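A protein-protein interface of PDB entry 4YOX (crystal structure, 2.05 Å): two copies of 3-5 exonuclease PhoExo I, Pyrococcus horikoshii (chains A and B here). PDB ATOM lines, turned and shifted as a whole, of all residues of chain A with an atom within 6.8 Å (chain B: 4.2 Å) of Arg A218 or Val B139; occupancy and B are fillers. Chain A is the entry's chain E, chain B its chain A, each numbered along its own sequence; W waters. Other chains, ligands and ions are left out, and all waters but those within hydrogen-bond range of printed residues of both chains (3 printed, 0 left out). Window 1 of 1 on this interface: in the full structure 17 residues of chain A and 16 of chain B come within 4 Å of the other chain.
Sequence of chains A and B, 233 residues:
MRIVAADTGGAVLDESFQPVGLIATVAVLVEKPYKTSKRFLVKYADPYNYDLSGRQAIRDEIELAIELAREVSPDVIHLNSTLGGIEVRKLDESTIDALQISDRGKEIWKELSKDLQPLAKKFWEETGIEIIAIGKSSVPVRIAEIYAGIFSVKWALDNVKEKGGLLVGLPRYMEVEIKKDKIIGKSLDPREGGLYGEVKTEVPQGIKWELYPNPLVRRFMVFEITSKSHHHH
No position is printed for both chains.
Hydrophobic or aromatic side chains of chain A that line the printed part of chain B: Pro A213, Pro A215 and Met A221. Of the 11 printed residues of chain B, 8 touch a printed residue of chain A. Printed residues of chain B that touch a printed residue of chain A: Tyr B34, Lys B136, Ser B137, Ser B138, Val B139, Pro B140, Arg B142 and Glu B192. Along chain B the printed residues that touch a printed residue of chain A span positions 34 to 192. Among the printed residues, 17 pairs touch across the chains.
O of Lys B136 sits close to NH2 of Arg A218 (3.2 Å). O of Leu A216 is in hydrogen-bond range of OG of Ser B137 (2.8 Å). O of Ser B137 sits at hydrogen-bond distance from N of Val A217, at 3.4 Å. The backbone NH (N) of Arg A218 sits at hydrogen-bond distance from the backbone carbonyl oxygen (O) of Ser B137, at 2.9 Å. The guanidinium group (NH2) of Arg A218 lies within hydrogen-bond range of the backbone carbonyl oxygen (O) of Ser B138 (3.2 Å). The backbone NH (N) of Val B139 is in hydrogen-bond range of the backbone carbonyl oxygen (O) of Pro A215, 2.9 Å away. The side-chain carboxylate of Glu B192 is in salt-bridge range of the guanidinium group of Arg A218 (3.6 Å).
The side-chain hydroxyl of Ser B138 sits at hydrogen-bond distance from the backbone NH of Val B141, at 3.0 Å. OE2 of Glu B192 is in salt-bridge range of NE of Arg B142, at 2.9 Å. N of Tyr A173 is in hydrogen-bond range of O of Arg A219 (2.8 Å). The side-chain amide oxygen (OD1) of Asn A214 lies within hydrogen-bond range of the backbone NH (N) of Leu A216, at 2.9 Å. OD1 of Asn A214 sits at hydrogen-bond distance from N of Val A217. The backbone NH of Asn A214 sits at hydrogen-bond distance from the backbone carbonyl oxygen of Phe A220 (2.8 Å).
Water W3 lies within hydrogen-bond range of NH1 of Arg A219 (2.8 Å) and OE1 of Glu B192 (2.9 Å). Water W1 lies within hydrogen-bond range of O of Glu B192 (2.8 Å) and N of Arg A219 (2.8 Å). Water W2 bridges OE1 of Glu B192 and NH1 of Arg A218.
Among the printed residues, merely in contact across the chains: Pro A213 with Tyr B34 (3.7 Å), Pro A213 with Glu B192 (3.8 Å), Asn A214 with Val B139 (3.3 Å), Pro A215 with Tyr B34 (3.7 Å), Pro A215 with Ser B138 (3.8 Å), Pro A215 with Pro B140 (3.2 Å), Arg A218 with Val B139 (3.8 Å), Arg A218 with Arg B142 (3.4 Å), Arg A219 with Glu B192 (3.99 Å) and Met A221 with Glu B192 (3.7 Å).
Of chain B, only Lys B136, Ser B137, Ser B138, Val B139, Arg B142 and Glu B192 come within 4 Å of Arg A218. Printed residues of chain A within 4 Å of Tyr B34: Pro A213 and Pro A215. Of the printed residues of chain B, Leu A216 touches Ser B137. Val B141 touches none of the printed residues of chain A.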
ATOM      1  N   TYR A 173     -34.276  19.479  -3.377  1.00  0.00           N
ATOM      2  CA  TYR A 173     -33.190  18.497  -3.489  1.00  0.00           C
ATOM      3  C   TYR A 173     -33.088  17.740  -4.812  1.00  0.00           C
ATOM      4  O   TYR A 173     -33.303  16.517  -4.903  1.00  0.00           O
ATOM      5  CB  TYR A 173     -33.244  17.508  -2.323  1.00  0.00           C
ATOM      6  CG  TYR A 173     -34.606  17.030  -1.896  1.00  0.00           C
ATOM      7  CD1 TYR A 173     -35.151  15.869  -2.437  1.00  0.00           C
ATOM      8  CD2 TYR A 173     -35.318  17.690  -0.891  1.00  0.00           C
ATOM      9  CE1 TYR A 173     -36.390  15.402  -2.021  1.00  0.00           C
ATOM     10  CE2 TYR A 173     -36.556  17.230  -0.468  1.00  0.00           C
ATOM     11  CZ  TYR A 173     -37.084  16.080  -1.040  1.00  0.00           C
ATOM     12  OH  TYR A 173     -38.314  15.611  -0.653  1.00  0.00           O
ATOM     13  N   PRO A 213     -25.627  24.898  -2.907  1.00  0.00           N
ATOM     14  CA  PRO A 213     -26.766  25.074  -2.000  1.00  0.00           C
ATOM     15  C   PRO A 213     -27.248  26.511  -1.873  1.00  0.00           C
ATOM     16  O   PRO A 213     -26.440  27.421  -1.681  1.00  0.00           O
ATOM     17  CB  PRO A 213     -26.216  24.604  -0.645  1.00  0.00           C
ATOM     18  CG  PRO A 213     -25.090  23.662  -0.998  1.00  0.00           C
ATOM     19  CD  PRO A 213     -24.476  24.272  -2.229  1.00  0.00           C
ATOM     20  N   ASN A 214     -28.558  26.701  -1.980  1.00  0.00           N
ATOM     21  CA  ASN A 214     -29.181  27.936  -1.550  1.00  0.00           C
ATOM     22  C   ASN A 214     -28.917  28.109  -0.048  1.00  0.00           C
ATOM     23  O   ASN A 214     -29.394  27.316   0.759  1.00  0.00           O
ATOM     24  CB  ASN A 214     -30.680  27.901  -1.847  1.00  0.00           C
ATOM     25  CG  ASN A 214     -31.364  29.250  -1.613  1.00  0.00           C
ATOM     26  OD1 ASN A 214     -30.994  30.003  -0.721  1.00  0.00           O
ATOM     27  ND2 ASN A 214     -32.374  29.542  -2.418  1.00  0.00           N
ATOM     28  N   PRO A 215     -28.161  29.148   0.338  1.00  0.00           N
ATOM     29  CA  PRO A 215     -27.787  29.252   1.755  1.00  0.00           C
ATOM     30  C   PRO A 215     -28.965  29.612   2.650  1.00  0.00           C
ATOM     31  O   PRO A 215     -28.871  29.416   3.861  1.00  0.00           O
ATOM     32  CB  PRO A 215     -26.734  30.351   1.773  1.00  0.00           C
ATOM     33  CG  PRO A 215     -27.048  31.198   0.522  1.00  0.00           C
ATOM     34  CD  PRO A 215     -27.564  30.211  -0.497  1.00  0.00           C
ATOM     35  N   LEU A 216     -30.057  30.101   2.067  1.00  0.00           N
ATOM     36  CA  LEU A 216     -31.217  30.541   2.844  1.00  0.00           C
ATOM     37  C   LEU A 216     -32.328  29.488   2.896  1.00  0.00           C
ATOM     38  O   LEU A 216     -33.301  29.642   3.637  1.00  0.00           O
ATOM     39  CB  LEU A 216     -31.786  31.859   2.265  1.00  0.00           C
ATOM     40  CG  LEU A 216     -30.783  33.005   2.155  1.00  0.00           C
ATOM     41  CD1 LEU A 216     -31.448  34.331   1.714  1.00  0.00           C
ATOM     42  CD2 LEU A 216     -30.052  33.204   3.480  1.00  0.00           C
ATOM     43  N   VAL A 217     -32.202  28.446   2.079  1.00  0.00           N
ATOM     44  CA  VAL A 217     -33.240  27.424   1.943  1.00  0.00           C
ATOM     45  C   VAL A 217     -32.607  26.034   1.876  1.00  0.00           C
ATOM     46  O   VAL A 217     -32.372  25.483   0.791  1.00  0.00           O
ATOM     47  CB  VAL A 217     -34.112  27.633   0.668  1.00  0.00           C
ATOM     48  CG1 VAL A 217     -35.412  26.854   0.798  1.00  0.00           C
ATOM     49  CG2 VAL A 217     -34.412  29.121   0.408  1.00  0.00           C
ATOM     50  N   ARG A 218     -32.341  25.470   3.045  1.00  0.00           N
ATOM     51  CA  ARG A 218     -31.632  24.207   3.148  1.00  0.00           C
ATOM     52  C   ARG A 218     -32.288  23.131   2.283  1.00  0.00           C
ATOM     53  O   ARG A 218     -33.522  23.081   2.201  1.00  0.00           O
ATOM     54  CB  ARG A 218     -31.598  23.765   4.608  1.00  0.00           C
ATOM     55  CG  ARG A 218     -30.718  22.564   4.834  1.00  0.00           C
ATOM     56  CD  ARG A 218     -30.115  22.626   6.235  1.00  0.00           C
ATOM     57  NE  ARG A 218     -30.966  22.070   7.281  1.00  0.00           N
ATOM     58  CZ  ARG A 218     -30.954  22.462   8.554  1.00  0.00           C
ATOM     59  NH1 ARG A 218     -31.747  21.858   9.429  1.00  0.00           N
ATOM     60  NH2 ARG A 218     -30.179  23.472   8.951  1.00  0.00           N
ATOM     61  N   ARG A 219     -31.462  22.309   1.624  1.00  0.00           N
ATOM     62  CA  ARG A 219     -31.900  21.235   0.727  1.00  0.00           C
ATOM     63  C   ARG A 219     -32.463  21.738  -0.613  1.00  0.00           C
ATOM     64  O   ARG A 219     -33.041  20.961  -1.381  1.00  0.00           O
ATOM     65  CB  ARG A 219     -32.929  20.317   1.406  1.00  0.00           C
ATOM     66  CG  ARG A 219     -32.382  19.543   2.607  1.00  0.00           C
ATOM     67  CD  ARG A 219     -33.395  18.514   3.103  1.00  0.00           C
ATOM     68  NE  ARG A 219     -34.599  19.180   3.578  1.00  0.00           N
ATOM     69  CZ  ARG A 219     -34.763  19.602   4.829  1.00  0.00           C
ATOM     70  NH1 ARG A 219     -33.816  19.386   5.741  1.00  0.00           N
ATOM     71  NH2 ARG A 219     -35.886  20.213   5.177  1.00  0.00           N
ATOM     72  N   PHE A 220     -32.326  23.032  -0.885  1.00  0.00           N
ATOM     73  CA  PHE A 220     -32.575  23.544  -2.234  1.00  0.00           C
ATOM     74  C   PHE A 220     -31.268  24.022  -2.863  1.00  0.00           C
ATOM     75  O   PHE A 220     -30.460  24.679  -2.207  1.00  0.00           O
ATOM     76  CB  PHE A 220     -33.591  24.683  -2.226  1.00  0.00           C
ATOM     77  CG  PHE A 220     -35.009  24.248  -1.955  1.00  0.00           C
ATOM     78  CD1 PHE A 220     -35.399  23.836  -0.688  1.00  0.00           C
ATOM     79  CD2 PHE A 220     -35.963  24.295  -2.965  1.00  0.00           C
ATOM     80  CE1 PHE A 220     -36.711  23.469  -0.434  1.00  0.00           C
ATOM     81  CE2 PHE A 220     -37.276  23.926  -2.723  1.00  0.00           C
ATOM     82  CZ  PHE A 220     -37.652  23.521  -1.450  1.00  0.00           C
ATOM     83  N   MET A 221     -31.066  23.696  -4.136  1.00  0.00           N
ATOM     84  CA  MET A 221     -29.845  24.078  -4.825  1.00  0.00           C
ATOM     85  C   MET A 221     -30.073  25.295  -5.715  1.00  0.00           C
ATOM     86  O   MET A 221     -31.196  25.561  -6.166  1.00  0.00           O
ATOM     87  CB  MET A 221     -29.302  22.907  -5.669  1.00  0.00           C
ATOM     88  CG  MET A 221     -29.053  21.620  -4.887  1.00  0.00           C
ATOM     89  SD  MET A 221     -27.809  21.793  -3.578  1.00  0.00           S
ATOM     90  CE  MET A 221     -28.754  21.416  -2.096  1.00  0.00           C
ATOM     91  N   TYR B  34     -21.078  27.863  -0.171  1.00  0.00           N
ATOM     92  CA  TYR B  34     -21.978  27.572   0.950  1.00  0.00           C
ATOM     93  C   TYR B  34     -22.031  26.065   1.271  1.00  0.00           C
ATOM     94  O   TYR B  34     -23.100  25.503   1.565  1.00  0.00           O
ATOM     95  CB  TYR B  34     -23.393  28.109   0.658  1.00  0.00           C
ATOM     96  CG  TYR B  34     -23.409  29.555   0.141  1.00  0.00           C
ATOM     97  CD1 TYR B  34     -23.169  30.635   0.997  1.00  0.00           C
ATOM     98  CD2 TYR B  34     -23.641  29.829  -1.202  1.00  0.00           C
ATOM     99  CE1 TYR B  34     -23.177  31.942   0.528  1.00  0.00           C
ATOM    100  CE2 TYR B  34     -23.651  31.130  -1.683  1.00  0.00           C
ATOM    101  CZ  TYR B  34     -23.414  32.182  -0.818  1.00  0.00           C
ATOM    102  OH  TYR B  34     -23.417  33.468  -1.312  1.00  0.00           O
ATOM    103  N   LYS B 136     -33.699  26.111  11.108  1.00  0.00           N
ATOM    104  CA  LYS B 136     -33.605  24.940  10.231  1.00  0.00           C
ATOM    105  C   LYS B 136     -33.468  25.272   8.751  1.00  0.00           C
ATOM    106  O   LYS B 136     -33.027  24.462   7.957  1.00  0.00           O
ATOM    107  CB  LYS B 136     -34.823  24.030  10.430  1.00  0.00           C
ATOM    108  CG  LYS B 136     -34.838  23.292  11.764  1.00  0.00           C
ATOM    109  CD  LYS B 136     -36.155  22.546  11.971  1.00  0.00           C
ATOM    110  CE  LYS B 136     -36.127  21.700  13.243  1.00  0.00           C
ATOM    111  NZ  LYS B 136     -37.494  21.449  13.792  1.00  0.00           N
ATOM    112  N   SER B 137     -33.899  26.461   8.380  1.00  0.00           N
ATOM    113  CA  SER B 137     -33.899  26.850   6.989  1.00  0.00           C
ATOM    114  C   SER B 137     -32.489  27.232   6.517  1.00  0.00           C
ATOM    115  O   SER B 137     -32.225  27.293   5.321  1.00  0.00           O
ATOM    116  CB  SER B 137     -34.890  28.002   6.793  1.00  0.00           C
ATOM    117  OG  SER B 137     -35.035  28.295   5.426  1.00  0.00           O
ATOM    118  N   SER B 138     -31.578  27.473   7.455  1.00  0.00           N
ATOM    119  CA  SER B 138     -30.276  28.038   7.106  1.00  0.00           C
ATOM    120  C   SER B 138     -29.205  26.991   6.795  1.00  0.00           C
ATOM    121  O   SER B 138     -28.974  26.077   7.575  1.00  0.00           O
ATOM    122  CB  SER B 138     -29.799  28.952   8.238  1.00  0.00           C
ATOM    123  OG  SER B 138     -28.441  29.334   8.082  1.00  0.00           O
ATOM    124  N   VAL B 139     -28.534  27.122   5.654  1.00  0.00           N
ATOM    125  CA  VAL B 139     -27.385  26.256   5.411  1.00  0.00           C
ATOM    126  C   VAL B 139     -26.169  26.626   6.282  1.00  0.00           C
ATOM    127  O   VAL B 139     -25.543  25.739   6.842  1.00  0.00           O
ATOM    128  CB  VAL B 139     -26.995  26.218   3.904  1.00  0.00           C
ATOM    129  CG1 VAL B 139     -25.662  25.514   3.719  1.00  0.00           C
ATOM    130  CG2 VAL B 139     -28.069  25.462   3.131  1.00  0.00           C
ATOM    131  N   PRO B 140     -25.838  27.920   6.424  1.00  0.00           N
ATOM    132  CA  PRO B 140     -24.750  28.226   7.370  1.00  0.00           C
ATOM    133  C   PRO B 140     -24.976  27.693   8.808  1.00  0.00           C
ATOM    134  O   PRO B 140     -24.011  27.298   9.470  1.00  0.00           O
ATOM    135  CB  PRO B 140     -24.710  29.758   7.350  1.00  0.00           C
ATOM    136  CG  PRO B 140     -25.119  30.087   5.935  1.00  0.00           C
ATOM    137  CD  PRO B 140     -26.205  29.108   5.618  1.00  0.00           C
ATOM    138  N   VAL B 141     -26.213  27.680   9.296  1.00  0.00           N
ATOM    139  CA  VAL B 141     -26.462  27.092  10.614  1.00  0.00           C
ATOM    140  C   VAL B 141     -26.114  25.597  10.628  1.00  0.00           C
ATOM    141  O   VAL B 141     -25.494  25.099  11.581  1.00  0.00           O
ATOM    142  CB  VAL B 141     -27.930  27.294  11.064  1.00  0.00           C
ATOM    143  CG1 VAL B 141     -28.274  26.347  12.190  1.00  0.00           C
ATOM    144  CG2 VAL B 141     -28.193  28.813  11.490  1.00  0.00           C
ATOM    145  N   ARG B 142     -26.484  24.889   9.563  1.00  0.00           N
ATOM    146  CA  ARG B 142     -26.187  23.461   9.469  1.00  0.00           C
ATOM    147  C   ARG B 142     -24.677  23.222   9.393  1.00  0.00           C
ATOM    148  O   ARG B 142     -24.165  22.261   9.963  1.00  0.00           O
ATOM    149  CB  ARG B 142     -26.884  22.840   8.257  1.00  0.00           C
ATOM    150  CG  ARG B 142     -26.497  21.377   7.982  1.00  0.00           C
ATOM    151  CD  ARG B 142     -26.811  20.437   9.140  1.00  0.00           C
ATOM    152  NE  ARG B 142     -26.632  19.038   8.707  1.00  0.00           N
ATOM    153  CZ  ARG B 142     -26.545  17.991   9.520  1.00  0.00           C
ATOM    154  NH1 ARG B 142     -26.571  18.156  10.849  1.00  0.00           N
ATOM    155  NH2 ARG B 142     -26.396  16.777   8.996  1.00  0.00           N
ATOM    156  N   ILE B 143     -23.957  24.104   8.712  1.00  0.00           N
ATOM    157  CA  ILE B 143     -22.501  23.997   8.696  1.00  0.00           C
ATOM    158  C   ILE B 143     -21.929  24.271  10.097  1.00  0.00           C
ATOM    159  O   ILE B 143     -20.967  23.625  10.512  1.00  0.00           O
ATOM    160  CB  ILE B 143     -21.891  24.952   7.681  1.00  0.00           C
ATOM    161  CG1 ILE B 143     -22.212  24.486   6.253  1.00  0.00           C
ATOM    162  CG2 ILE B 143     -20.382  25.073   7.885  1.00  0.00           C
ATOM    163  CD1 ILE B 143     -21.942  25.583   5.197  1.00  0.00           C
ATOM    164  N   GLU B 192     -28.746  17.788   1.276  1.00  0.00           N
ATOM    165  CA  GLU B 192     -28.204  19.088   1.689  1.00  0.00           C
ATOM    166  C   GLU B 192     -27.128  19.573   0.729  1.00  0.00           C
ATOM    167  O   GLU B 192     -26.673  20.716   0.837  1.00  0.00           O
ATOM    168  CB  GLU B 192     -27.661  19.024   3.122  1.00  0.00           C
ATOM    169  CG  GLU B 192     -28.770  18.805   4.134  1.00  0.00           C
ATOM    170  CD  GLU B 192     -28.307  18.770   5.602  1.00  0.00           C
ATOM    171  OE1 GLU B 192     -29.166  19.068   6.461  1.00  0.00           O
ATOM    172  OE2 GLU B 192     -27.134  18.410   5.903  1.00  0.00           O
ATOM    173  N   LEU B 195     -22.613  19.155   2.496  1.00  0.00           N
ATOM    174  CA  LEU B 195     -22.089  20.040   3.525  1.00  0.00           C
ATOM    175  C   LEU B 195     -21.012  19.343   4.351  1.00  0.00           C
ATOM    176  O   LEU B 195     -21.166  18.183   4.725  1.00  0.00           O
ATOM    177  CB  LEU B 195     -23.228  20.522   4.412  1.00  0.00           C
ATOM    178  CG  LEU B 195     -24.378  21.149   3.625  1.00  0.00           C
ATOM    179  CD1 LEU B 195     -25.505  21.616   4.550  1.00  0.00           C
ATOM    180  CD2 LEU B 195     -23.874  22.311   2.724  1.00  0.00           C
HETATM  181  O   HOH W   1     -28.648  22.450   1.830  1.00  0.00           O
HETATM  182  O   HOH W   2     -30.542  19.307   8.928  1.00  0.00           O
HETATM  183  O   HOH W   3     -31.616  17.678   5.999  1.00  0.00           O
